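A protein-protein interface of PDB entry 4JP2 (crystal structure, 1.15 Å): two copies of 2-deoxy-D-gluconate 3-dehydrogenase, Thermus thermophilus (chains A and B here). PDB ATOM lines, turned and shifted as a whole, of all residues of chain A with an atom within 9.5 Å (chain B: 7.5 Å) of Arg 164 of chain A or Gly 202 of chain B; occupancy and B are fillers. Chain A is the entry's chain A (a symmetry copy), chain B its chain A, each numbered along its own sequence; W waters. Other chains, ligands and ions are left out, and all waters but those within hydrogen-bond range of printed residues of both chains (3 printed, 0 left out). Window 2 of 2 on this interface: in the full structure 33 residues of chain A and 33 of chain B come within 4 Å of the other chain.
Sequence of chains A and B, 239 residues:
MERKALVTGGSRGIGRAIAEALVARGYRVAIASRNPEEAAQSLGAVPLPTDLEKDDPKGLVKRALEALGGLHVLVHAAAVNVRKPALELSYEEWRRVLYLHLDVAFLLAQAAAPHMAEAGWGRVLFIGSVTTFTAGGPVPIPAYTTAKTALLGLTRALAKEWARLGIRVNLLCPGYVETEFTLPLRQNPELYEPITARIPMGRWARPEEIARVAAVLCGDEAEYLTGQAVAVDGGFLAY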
ATOM      1  N   MET A 116     -26.056   8.442 -24.565  1.00  0.00           N
ATOM      2  CA  MET A 116     -26.406   9.657 -23.844  1.00  0.00           C
ATOM      3  C   MET A 116     -26.827  10.714 -24.857  1.00  0.00           C
ATOM      4  O   MET A 116     -27.797  11.444 -24.644  1.00  0.00           O
ATOM      5  CB  MET A 116     -25.208  10.169 -23.053  1.00  0.00           C
ATOM      6  CG  MET A 116     -24.745   9.235 -21.966  1.00  0.00           C
ATOM      7  SD  MET A 116     -23.048   9.773 -21.279  1.00  0.00           S
ATOM      8  CE  MET A 116     -22.948   8.538 -19.797  1.00  0.00           C
ATOM      9  N   ALA A 117     -26.096  10.788 -25.965  1.00  0.00           N
ATOM     10  CA  ALA A 117     -26.391  11.759 -27.008  1.00  0.00           C
ATOM     11  C   ALA A 117     -27.782  11.528 -27.585  1.00  0.00           C
ATOM     12  O   ALA A 117     -28.526  12.477 -27.834  1.00  0.00           O
ATOM     13  CB  ALA A 117     -25.342  11.677 -28.109  1.00  0.00           C
ATOM     14  N   GLU A 118     -28.134  10.263 -27.795  1.00  0.00           N
ATOM     15  CA  GLU A 118     -29.444   9.925 -28.334  1.00  0.00           C
ATOM     16  C   GLU A 118     -30.539  10.373 -27.372  1.00  0.00           C
ATOM     17  O   GLU A 118     -31.604  10.827 -27.794  1.00  0.00           O
ATOM     18  CB  GLU A 118     -29.548   8.416 -28.576  1.00  0.00           C
ATOM     19  CG  GLU A 118     -30.896   7.972 -29.128  1.00  0.00           C
ATOM     20  CD  GLU A 118     -30.930   6.499 -29.481  1.00  0.00           C
ATOM     21  OE1 GLU A 118     -30.683   5.665 -28.585  1.00  0.00           O
ATOM     22  OE2 GLU A 118     -31.206   6.175 -30.656  1.00  0.00           O
ATOM     23  N   GLY A 120     -30.209  12.836 -25.322  1.00  0.00           N
ATOM     24  CA  GLY A 120     -30.138  14.282 -25.203  1.00  0.00           C
ATOM     25  C   GLY A 120     -29.758  14.754 -23.809  1.00  0.00           C
ATOM     26  O   GLY A 120     -29.957  15.921 -23.470  1.00  0.00           O
ATOM     27  N   TRP A 121     -29.197  13.854 -23.006  1.00  0.00           N
ATOM     28  CA  TRP A 121     -28.806  14.179 -21.636  1.00  0.00           C
ATOM     29  C   TRP A 121     -27.840  13.112 -21.144  1.00  0.00           C
ATOM     30  O   TRP A 121     -28.123  11.917 -21.246  1.00  0.00           O
ATOM     31  CB  TRP A 121     -30.047  14.183 -20.739  1.00  0.00           C
ATOM     32  CG  TRP A 121     -29.857  14.761 -19.362  1.00  0.00           C
ATOM     33  CD1 TRP A 121     -30.199  16.020 -18.952  1.00  0.00           C
ATOM     34  CD2 TRP A 121     -29.353  14.086 -18.199  1.00  0.00           C
ATOM     35  NE1 TRP A 121     -29.951  16.167 -17.610  1.00  0.00           N
ATOM     36  CE2 TRP A 121     -29.432  14.997 -17.122  1.00  0.00           C
ATOM     37  CE3 TRP A 121     -28.847  12.800 -17.961  1.00  0.00           C
ATOM     38  CZ2 TRP A 121     -29.025  14.665 -15.828  1.00  0.00           C
ATOM     39  CZ3 TRP A 121     -28.442  12.470 -16.667  1.00  0.00           C
ATOM     40  CH2 TRP A 121     -28.536  13.401 -15.620  1.00  0.00           C
ATOM     41  N   GLY A 122     -26.701  13.537 -20.612  1.00  0.00           N
ATOM     42  CA  GLY A 122     -25.745  12.575 -20.111  1.00  0.00           C
ATOM     43  C   GLY A 122     -24.814  13.164 -19.077  1.00  0.00           C
ATOM     44  O   GLY A 122     -24.593  14.381 -19.026  1.00  0.00           O
ATOM     45  N   LEU A 158     -13.161  15.407 -23.360  1.00  0.00           N
ATOM     46  CA  LEU A 158     -14.481  14.859 -23.638  1.00  0.00           C
ATOM     47  C   LEU A 158     -15.573  15.885 -23.352  1.00  0.00           C
ATOM     48  O   LEU A 158     -16.576  15.943 -24.063  1.00  0.00           O
ATOM     49  CB  LEU A 158     -14.711  13.578 -22.832  1.00  0.00           C
ATOM     50  CG  LEU A 158     -13.705  12.452 -23.116  1.00  0.00           C
ATOM     51  CD1 LEU A 158     -14.112  11.208 -22.348  1.00  0.00           C
ATOM     52  CD2 LEU A 158     -13.647  12.152 -24.610  1.00  0.00           C
ATOM     53  N   ALA A 159     -15.387  16.697 -22.316  1.00  0.00           N
ATOM     54  CA  ALA A 159     -16.369  17.728 -22.002  1.00  0.00           C
ATOM     55  C   ALA A 159     -16.494  18.663 -23.205  1.00  0.00           C
ATOM     56  O   ALA A 159     -17.599  19.040 -23.599  1.00  0.00           O
ATOM     57  CB  ALA A 159     -15.937  18.514 -20.774  1.00  0.00           C
ATOM     58  N   LYS A 160     -15.361  19.027 -23.792  1.00  0.00           N
ATOM     59  CA  LYS A 160     -15.370  19.915 -24.944  1.00  0.00           C
ATOM     60  C   LYS A 160     -16.067  19.275 -26.141  1.00  0.00           C
ATOM     61  O   LYS A 160     -16.932  19.886 -26.767  1.00  0.00           O
ATOM     62  CB  LYS A 160     -13.941  20.291 -25.346  1.00  0.00           C
ATOM     63  CG  LYS A 160     -13.887  21.304 -26.481  1.00  0.00           C
ATOM     64  CD  LYS A 160     -12.479  21.508 -27.026  1.00  0.00           C
ATOM     65  CE  LYS A 160     -11.994  20.295 -27.808  1.00  0.00           C
ATOM     66  NZ  LYS A 160     -10.705  20.569 -28.505  1.00  0.00           N
ATOM     67  N   GLU A 161     -15.695  18.037 -26.442  1.00  0.00           N
ATOM     68  CA  GLU A 161     -16.250  17.328 -27.588  1.00  0.00           C
ATOM     69  C   GLU A 161     -17.740  17.031 -27.523  1.00  0.00           C
ATOM     70  O   GLU A 161     -18.432  17.098 -28.544  1.00  0.00           O
ATOM     71  CB  GLU A 161     -15.500  16.002 -27.794  1.00  0.00           C
ATOM     72  CG  GLU A 161     -15.886  15.241 -29.067  1.00  0.00           C
ATOM     73  CD  GLU A 161     -15.153  13.913 -29.212  1.00  0.00           C
ATOM     74  OE1 GLU A 161     -13.930  13.884 -28.943  1.00  0.00           O
ATOM     75  OE2 GLU A 161     -15.793  12.905 -29.607  1.00  0.00           O
ATOM     76  N   TRP A 162     -18.239  16.721 -26.333  1.00  0.00           N
ATOM     77  CA  TRP A 162     -19.637  16.333 -26.194  1.00  0.00           C
ATOM     78  C   TRP A 162     -20.594  17.351 -25.593  1.00  0.00           C
ATOM     79  O   TRP A 162     -21.764  17.044 -25.358  1.00  0.00           O
ATOM     80  CB  TRP A 162     -19.708  15.024 -25.402  1.00  0.00           C
ATOM     81  CG  TRP A 162     -18.878  13.930 -26.015  1.00  0.00           C
ATOM     82  CD1 TRP A 162     -18.526  13.809 -27.330  1.00  0.00           C
ATOM     83  CD2 TRP A 162     -18.329  12.787 -25.348  1.00  0.00           C
ATOM     84  NE1 TRP A 162     -17.791  12.665 -27.524  1.00  0.00           N
ATOM     85  CE2 TRP A 162     -17.656  12.018 -26.325  1.00  0.00           C
ATOM     86  CE3 TRP A 162     -18.341  12.335 -24.023  1.00  0.00           C
ATOM     87  CZ2 TRP A 162     -17.001  10.822 -26.015  1.00  0.00           C
ATOM     88  CZ3 TRP A 162     -17.688  11.144 -23.716  1.00  0.00           C
ATOM     89  CH2 TRP A 162     -17.028  10.403 -24.711  1.00  0.00           C
ATOM     90  N   ALA A 163     -20.114  18.569 -25.374  1.00  0.00           N
ATOM     91  CA  ALA A 163     -20.936  19.614 -24.782  1.00  0.00           C
ATOM     92  C   ALA A 163     -22.263  19.850 -25.507  1.00  0.00           C
ATOM     93  O   ALA A 163     -23.310  19.971 -24.867  1.00  0.00           O
ATOM     94  CB  ALA A 163     -20.146  20.914 -24.708  1.00  0.00           C
ATOM     95  N   ARG A 164     -22.224  19.902 -26.835  1.00  0.00           N
ATOM     96  CA  ARG A 164     -23.437  20.148 -27.612  1.00  0.00           C
ATOM     97  C   ARG A 164     -24.350  18.931 -27.725  1.00  0.00           C
ATOM     98  O   ARG A 164     -25.436  19.021 -28.302  1.00  0.00           O
ATOM     99  CB  ARG A 164     -23.076  20.647 -29.013  1.00  0.00           C
ATOM    100  CG  ARG A 164     -22.330  21.974 -29.045  1.00  0.00           C
ATOM    101  CD  ARG A 164     -23.160  23.106 -28.461  1.00  0.00           C
ATOM    102  NE  ARG A 164     -22.637  24.415 -28.843  1.00  0.00           N
ATOM    103  CZ  ARG A 164     -22.639  24.884 -30.087  1.00  0.00           C
ATOM    104  NH1 ARG A 164     -23.138  24.151 -31.072  1.00  0.00           N
ATOM    105  NH2 ARG A 164     -22.140  26.084 -30.348  1.00  0.00           N
ATOM    106  N   LEU A 165     -23.917  17.802 -27.173  1.00  0.00           N
ATOM    107  CA  LEU A 165     -24.701  16.571 -27.213  1.00  0.00           C
ATOM    108  C   LEU A 165     -25.482  16.363 -25.920  1.00  0.00           C
ATOM    109  O   LEU A 165     -26.113  15.321 -25.732  1.00  0.00           O
ATOM    110  CB  LEU A 165     -23.789  15.364 -27.442  1.00  0.00           C
ATOM    111  CG  LEU A 165     -22.887  15.379 -28.676  1.00  0.00           C
ATOM    112  CD1 LEU A 165     -22.062  14.102 -28.711  1.00  0.00           C
ATOM    113  CD2 LEU A 165     -23.731  15.506 -29.936  1.00  0.00           C
ATOM    114  N   GLY A 166     -25.435  17.351 -25.030  1.00  0.00           N
ATOM    115  CA  GLY A 166     -26.151  17.255 -23.770  1.00  0.00           C
ATOM    116  C   GLY A 166     -25.405  16.507 -22.683  1.00  0.00           C
ATOM    117  O   GLY A 166     -25.948  16.257 -21.608  1.00  0.00           O
ATOM    118  N   ILE A 167     -24.152  16.158 -22.954  1.00  0.00           N
ATOM    119  CA  ILE A 167     -23.343  15.420 -21.997  1.00  0.00           C
ATOM    120  C   ILE A 167     -22.413  16.340 -21.210  1.00  0.00           C
ATOM    121  O   ILE A 167     -21.782  17.226 -21.785  1.00  0.00           O
ATOM    122  CB  ILE A 167     -22.473  14.361 -22.719  1.00  0.00           C
ATOM    123  CG1 ILE A 167     -23.359  13.412 -23.533  1.00  0.00           C
ATOM    124  CG2 ILE A 167     -21.658  13.574 -21.702  1.00  0.00           C
ATOM    125  CD1 ILE A 167     -22.588  12.465 -24.436  1.00  0.00           C
ATOM    126  N   ARG A 168     -22.348  16.137 -19.896  1.00  0.00           N
ATOM    127  CA  ARG A 168     -21.443  16.899 -19.038  1.00  0.00           C
ATOM    128  C   ARG A 168     -20.435  15.863 -18.539  1.00  0.00           C
ATOM    129  O   ARG A 168     -20.810  14.732 -18.214  1.00  0.00           O
ATOM    130  CB  ARG A 168     -22.190  17.536 -17.861  1.00  0.00           C
ATOM    131  CG  ARG A 168     -23.428  18.328 -18.264  1.00  0.00           C
ATOM    132  CD  ARG A 168     -23.111  19.415 -19.282  1.00  0.00           C
ATOM    133  NE  ARG A 168     -24.331  19.987 -19.854  1.00  0.00           N
ATOM    134  CZ  ARG A 168     -24.617  20.018 -21.153  1.00  0.00           C
ATOM    135  NH1 ARG A 168     -23.777  19.505 -22.040  1.00  0.00           N
ATOM    136  NH2 ARG A 168     -25.746  20.577 -21.568  1.00  0.00           N
ATOM    137  N   VAL A 169     -19.162  16.244 -18.506  1.00  0.00           N
ATOM    138  CA  VAL A 169     -18.089  15.347 -18.086  1.00  0.00           C
ATOM    139  C   VAL A 169     -17.251  16.048 -17.028  1.00  0.00           C
ATOM    140  O   VAL A 169     -16.719  17.129 -17.275  1.00  0.00           O
ATOM    141  CB  VAL A 169     -17.171  14.988 -19.283  1.00  0.00           C
ATOM    142  CG1 VAL A 169     -16.139  13.956 -18.857  1.00  0.00           C
ATOM    143  CG2 VAL A 169     -18.005  14.472 -20.453  1.00  0.00           C
ATOM    144  N   GLU A 223     -25.897  20.950 -14.861  1.00  0.00           N
ATOM    145  CA  GLU A 223     -26.247  21.318 -16.227  1.00  0.00           C
ATOM    146  C   GLU A 223     -25.237  22.241 -16.903  1.00  0.00           C
ATOM    147  O   GLU A 223     -24.929  22.049 -18.079  1.00  0.00           O
ATOM    148  CB  GLU A 223     -27.637  21.959 -16.259  1.00  0.00           C
ATOM    149  CG  GLU A 223     -28.051  22.574 -17.599  1.00  0.00           C
ATOM    150  CD  GLU A 223     -27.947  21.620 -18.773  1.00  0.00           C
ATOM    151  OE1 GLU A 223     -28.145  20.405 -18.573  1.00  0.00           O
ATOM    152  OE2 GLU A 223     -27.684  22.087 -19.904  1.00  0.00           O
ATOM    153  N   TYR A 224     -24.718  23.232 -16.178  1.00  0.00           N
ATOM    154  CA  TYR A 224     -23.750  24.164 -16.760  1.00  0.00           C
ATOM    155  C   TYR A 224     -22.345  23.943 -16.190  1.00  0.00           C
ATOM    156  O   TYR A 224     -21.474  24.808 -16.309  1.00  0.00           O
ATOM    157  CB  TYR A 224     -24.191  25.615 -16.505  1.00  0.00           C
ATOM    158  CG  TYR A 224     -23.667  26.613 -17.522  1.00  0.00           C
ATOM    159  CD1 TYR A 224     -24.155  26.626 -18.830  1.00  0.00           C
ATOM    160  CD2 TYR A 224     -22.671  27.529 -17.185  1.00  0.00           C
ATOM    161  CE1 TYR A 224     -23.664  27.524 -19.777  1.00  0.00           C
ATOM    162  CE2 TYR A 224     -22.173  28.432 -18.122  1.00  0.00           C
ATOM    163  CZ  TYR A 224     -22.671  28.424 -19.415  1.00  0.00           C
ATOM    164  OH  TYR A 224     -22.165  29.309 -20.342  1.00  0.00           O
ATOM    165  N   THR A 226     -19.169  21.597 -16.520  1.00  0.00           N
ATOM    166  CA  THR A 226     -18.535  20.559 -17.306  1.00  0.00           C
ATOM    167  C   THR A 226     -17.066  20.866 -17.579  1.00  0.00           C
ATOM    168  O   THR A 226     -16.662  22.032 -17.659  1.00  0.00           O
ATOM    169  CB  THR A 226     -19.312  20.341 -18.632  1.00  0.00           C
ATOM    170  OG1 THR A 226     -18.877  19.122 -19.238  1.00  0.00           O
ATOM    171  CG2 THR A 226     -19.109  21.506 -19.594  1.00  0.00           C
ATOM    172  N   TYR B 192     -18.900  39.388 -27.694  1.00  0.00           N
ATOM    173  CA  TYR B 192     -19.733  38.224 -27.422  1.00  0.00           C
ATOM    174  C   TYR B 192     -19.362  37.014 -28.271  1.00  0.00           C
ATOM    175  O   TYR B 192     -19.293  35.896 -27.761  1.00  0.00           O
ATOM    176  CB  TYR B 192     -21.210  38.579 -27.635  1.00  0.00           C
ATOM    177  CG  TYR B 192     -22.156  37.404 -27.508  1.00  0.00           C
ATOM    178  CD1 TYR B 192     -22.434  36.582 -28.600  1.00  0.00           C
ATOM    179  CD2 TYR B 192     -22.763  37.104 -26.288  1.00  0.00           C
ATOM    180  CE1 TYR B 192     -23.292  35.490 -28.482  1.00  0.00           C
ATOM    181  CE2 TYR B 192     -23.621  36.015 -26.158  1.00  0.00           C
ATOM    182  CZ  TYR B 192     -23.882  35.214 -27.258  1.00  0.00           C
ATOM    183  OH  TYR B 192     -24.728  34.135 -27.132  1.00  0.00           O
ATOM    184  N   THR B 196     -18.139  33.512 -26.686  1.00  0.00           N
ATOM    185  CA  THR B 196     -19.071  32.401 -26.834  1.00  0.00           C
ATOM    186  C   THR B 196     -18.480  31.248 -27.642  1.00  0.00           C
ATOM    187  O   THR B 196     -18.818  30.085 -27.413  1.00  0.00           O
ATOM    188  CB  THR B 196     -20.381  32.881 -27.488  1.00  0.00           C
ATOM    189  OG1 THR B 196     -20.924  33.961 -26.716  1.00  0.00           O
ATOM    190  CG2 THR B 196     -21.399  31.750 -27.540  1.00  0.00           C
ATOM    191  N   ALA B 197     -17.595  31.569 -28.581  1.00  0.00           N
ATOM    192  CA  ALA B 197     -16.959  30.546 -29.403  1.00  0.00           C
ATOM    193  C   ALA B 197     -16.084  29.636 -28.543  1.00  0.00           C
ATOM    194  O   ALA B 197     -15.737  28.529 -28.954  1.00  0.00           O
ATOM    195  CB  ALA B 197     -16.121  31.199 -30.494  1.00  0.00           C
ATOM    196  N   ARG B 198     -15.730  30.108 -27.350  1.00  0.00           N
ATOM    197  CA  ARG B 198     -14.896  29.338 -26.435  1.00  0.00           C
ATOM    198  C   ARG B 198     -15.704  28.589 -25.379  1.00  0.00           C
ATOM    199  O   ARG B 198     -15.136  27.912 -24.522  1.00  0.00           O
ATOM    200  CB  ARG B 198     -13.879  30.253 -25.761  1.00  0.00           C
ATOM    201  CG  ARG B 198     -12.838  30.796 -26.719  1.00  0.00           C
ATOM    202  CD  ARG B 198     -12.045  31.911 -26.076  1.00  0.00           C
ATOM    203  NE  ARG B 198     -11.381  31.472 -24.855  1.00  0.00           N
ATOM    204  CZ  ARG B 198     -10.735  32.288 -24.029  1.00  0.00           C
ATOM    205  NH1 ARG B 198     -10.671  33.586 -24.297  1.00  0.00           N
ATOM    206  NH2 ARG B 198     -10.154  31.809 -22.939  1.00  0.00           N
ATOM    207  N   ILE B 199     -17.026  28.720 -25.432  1.00  0.00           N
ATOM    208  CA  ILE B 199     -17.891  28.010 -24.491  1.00  0.00           C
ATOM    209  C   ILE B 199     -18.382  26.769 -25.235  1.00  0.00           C
ATOM    210  O   ILE B 199     -19.212  26.870 -26.137  1.00  0.00           O
ATOM    211  CB  ILE B 199     -19.125  28.851 -24.078  1.00  0.00           C
ATOM    212  CG1 ILE B 199     -18.687  30.182 -23.466  1.00  0.00           C
ATOM    213  CG2 ILE B 199     -19.966  28.070 -23.071  1.00  0.00           C
ATOM    214  CD1 ILE B 199     -19.843  31.123 -23.167  1.00  0.00           C
ATOM    215  N   PRO B 200     -17.868  25.583 -24.878  1.00  0.00           N
ATOM    216  CA  PRO B 200     -18.287  24.349 -25.551  1.00  0.00           C
ATOM    217  C   PRO B 200     -19.799  24.156 -25.632  1.00  0.00           C
ATOM    218  O   PRO B 200     -20.315  23.704 -26.652  1.00  0.00           O
ATOM    219  CB  PRO B 200     -17.598  23.264 -24.732  1.00  0.00           C
ATOM    220  CG  PRO B 200     -16.319  23.934 -24.321  1.00  0.00           C
ATOM    221  CD  PRO B 200     -16.802  25.307 -23.897  1.00  0.00           C
ATOM    222  N   MET B 201     -20.512  24.493 -24.564  1.00  0.00           N
ATOM    223  CA  MET B 201     -21.959  24.338 -24.574  1.00  0.00           C
ATOM    224  C   MET B 201     -22.650  25.300 -25.537  1.00  0.00           C
ATOM    225  O   MET B 201     -23.834  25.148 -25.824  1.00  0.00           O
ATOM    226  CB  MET B 201     -22.511  24.457 -23.154  1.00  0.00           C
ATOM    227  CG  MET B 201     -22.266  23.176 -22.366  1.00  0.00           C
ATOM    228  SD  MET B 201     -22.947  23.155 -20.578  1.00  0.00           S
ATOM    229  CE  MET B 201     -24.767  23.678 -20.964  1.00  0.00           C
ATOM    230  N   GLY B 202     -21.899  26.281 -26.037  1.00  0.00           N
ATOM    231  CA  GLY B 202     -22.424  27.219 -27.017  1.00  0.00           C
ATOM    232  C   GLY B 202     -23.479  28.212 -26.582  1.00  0.00           C
ATOM    233  O   GLY B 202     -24.172  28.790 -27.422  1.00  0.00           O
ATOM    234  N   ARG B 203     -23.603  28.427 -25.280  1.00  0.00           N
ATOM    235  CA  ARG B 203     -24.586  29.363 -24.764  1.00  0.00           C
ATOM    236  C   ARG B 203     -24.137  29.857 -23.407  1.00  0.00           C
ATOM    237  O   ARG B 203     -23.316  29.224 -22.743  1.00  0.00           O
ATOM    238  CB  ARG B 203     -25.952  28.684 -24.617  1.00  0.00           C
ATOM    239  CG  ARG B 203     -26.012  27.618 -23.518  1.00  0.00           C
ATOM    240  CD  ARG B 203     -27.415  27.033 -23.406  1.00  0.00           C
ATOM    241  NE  ARG B 203     -27.538  25.977 -22.400  1.00  0.00           N
ATOM    242  CZ  ARG B 203     -27.649  26.182 -21.090  1.00  0.00           C
ATOM    243  NH1 ARG B 203     -27.651  27.415 -20.600  1.00  0.00           N
ATOM    244  NH2 ARG B 203     -27.778  25.149 -20.269  1.00  0.00           N
ATOM    245  N   TRP B 204     -24.674  31.001 -23.008  1.00  0.00           N
ATOM    246  CA  TRP B 204     -24.377  31.578 -21.711  1.00  0.00           C
ATOM    247  C   TRP B 204     -25.330  30.920 -20.718  1.00  0.00           C
ATOM    248  O   TRP B 204     -26.356  30.363 -21.105  1.00  0.00           O
ATOM    249  CB  TRP B 204     -24.597  33.091 -21.755  1.00  0.00           C
ATOM    250  CG  TRP B 204     -23.514  33.820 -22.499  1.00  0.00           C
ATOM    251  CD1 TRP B 204     -22.913  33.436 -23.665  1.00  0.00           C
ATOM    252  CD2 TRP B 204     -22.888  35.044 -22.110  1.00  0.00           C
ATOM    253  NE1 TRP B 204     -21.948  34.347 -24.023  1.00  0.00           N
ATOM    254  CE2 TRP B 204     -21.912  35.345 -23.085  1.00  0.00           C
ATOM    255  CE3 TRP B 204     -23.056  35.918 -21.028  1.00  0.00           C
ATOM    256  CZ2 TRP B 204     -21.106  36.484 -23.012  1.00  0.00           C
ATOM    257  CZ3 TRP B 204     -22.253  37.051 -20.954  1.00  0.00           C
ATOM    258  CH2 TRP B 204     -21.290  37.321 -21.942  1.00  0.00           C
ATOM    259  N   GLY B 234     -19.955  26.138 -18.374  1.00  0.00           N
ATOM    260  CA  GLY B 234     -20.293  25.573 -19.669  1.00  0.00           C
ATOM    261  C   GLY B 234     -19.125  25.007 -20.454  1.00  0.00           C
ATOM    262  O   GLY B 234     -19.248  24.743 -21.657  1.00  0.00           O
HETATM  263  O   HOH W   1     -23.854  28.298 -30.395  1.00  0.00           O
HETATM  264  O   HOH W   2     -19.545  27.736 -28.965  1.00  0.00           O
HETATM  265  O   HOH W   3     -19.956  25.084 -29.029  1.00  0.00           O
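The guanidinium group (NE) of Arg 164 of chain A sits at hydrogen-bond distance from the backbone carbonyl oxygen (O) of Pro 200 of chain B (3.3 Å). NE of Arg 164 of chain A is in hydrogen-bond range of O of Met 201 of chain B (3.3 Å). The guanidinium group (NE) of Arg 168 of chain A sits at hydrogen-bond distance from the side-chain sulfur (SD) of Met 201 of chain B. NH2 of Arg 203 of chain B is in salt-bridge range of OE2 of Glu 223 of chain A (3.1 Å). The backbone carbonyl oxygen of Arg 203 of chain B is in hydrogen-bond range of the side-chain hydroxyl of Tyr 224 of chain A (2.7 Å). The backbone NH (N) of Gly 234 of chain B sits at hydrogen-bond distance from the backbone carbonyl oxygen (O) of Tyr 224 of chain A (2.9 Å). N of Gly 202 of chain B lies close to NE of Arg 164 of chain A. The side-chain sulfur (SD) of Met 201 of chain B lies close to the backbone carbonyl oxygen (O) of Glu 223 of chain A, 3.4 Å away.
The side-chain hydroxyl of Thr 196 of chain B sits at hydrogen-bond distance from the indole nitrogen of Trp 204 of chain B (2.9 Å). The backbone NH of Met 201 of chain B is in hydrogen-bond range of the backbone carbonyl oxygen of Gly 234 of chain B (3.2 Å). The backbone NH (N) of Arg 168 of chain A sits at hydrogen-bond distance from the backbone carbonyl oxygen (O) of Gly 122 of chain A (3.0 Å). O of Ala 163 of chain A lies within hydrogen-bond range of NH1 of Arg 168 of chain A, 2.9 Å away. The guanidinium group (NH2) of Arg 168 of chain A lies within salt-bridge range of the side-chain carboxylate (OE2) of Glu 223 of chain A. N of Val 169 of chain A is in hydrogen-bond range of OG1 of Thr 226 of chain A (3.0 Å).
Among the printed residues, merely in contact across the chains: Lys 160 of chain A with Pro 200 of chain B, Ala 163 of chain A with Pro 200 of chain B, Ala 163 of chain A with Met 201 of chain B, Tyr 224 of chain A with Ile 199 of chain B, Tyr 224 of chain A with Met 201 of chain B, Tyr 224 of chain A with Trp 204 of chain B and Thr 226 of chain A with Gly 234 of chain B.
Arg 164 of chain A touches just these residues of chain B: Pro 200 (3.3 Å), Met 201 (3.3 Å) and Gly 202 (3.4 Å). Of chain A, only Arg 164 (3.4 Å) comes within 4 Å of Gly 202 of chain B. Ala 163 of chain A touches just these residues of chain B: Pro 200 (3.4 Å) and Met 201 (3.6 Å). Of the printed residues of chain A, Pro 200 of chain B touches Lys 160, Ala 163 and Arg 164. Printed residues of chain A within 4 Å of Met 201 of chain B: Ala 163, Arg 164, Arg 168, Glu 223 and Tyr 224. Of the printed residues of chain B, Arg 168 of chain A touches Met 201. Printed residues of chain A within 4 Å of Trp 204 of chain B: Tyr 224 (3.5 Å). Gly 122 of chain A touches none of the printed residues of chain B. The nearest residue of chain B that does not touch Arg 164 of chain A is Ile 199 of chain B (5.0 Å).
Of the 21 printed residues of chain A, 7 touch a printed residue of chain B. Hydrophobic or aromatic side chains of chain A that line the printed part of chain B: Ala 163 and Tyr 224. Hydrophobic or aromatic side chains of chain B within 4 Å of the printed part of chain A: Ile 199, Pro 200 and Met 201. Among the printed residues, Asp or Glu carboxylates within 4 Å of a Lys or Arg side-chain nitrogen of the other chain: Glu 223 of chain A with Arg 203 of chain B.
No position is printed for both chains. Of the 15 pairs that touch across the chains among the printed residues, none has its exchanged pair printed and touching as well.
Water W3 lies within hydrogen-bond range of NH2 of Arg 164 of chain A (2.7 Å), O of Pro 200 of chain B (2.8 Å) and O of Ile 199 of chain B (3.5 Å). Water W1 lies within hydrogen-bond range of the guanidinium group (NH2) of Arg 164 of chain A and the backbone carbonyl oxygen (O) of Gly 202 of chain B. Water W2 lies within hydrogen-bond range of O of Thr 196 of chain B, O of Ile 199 of chain B and NH2 of Arg 164 of chain A.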
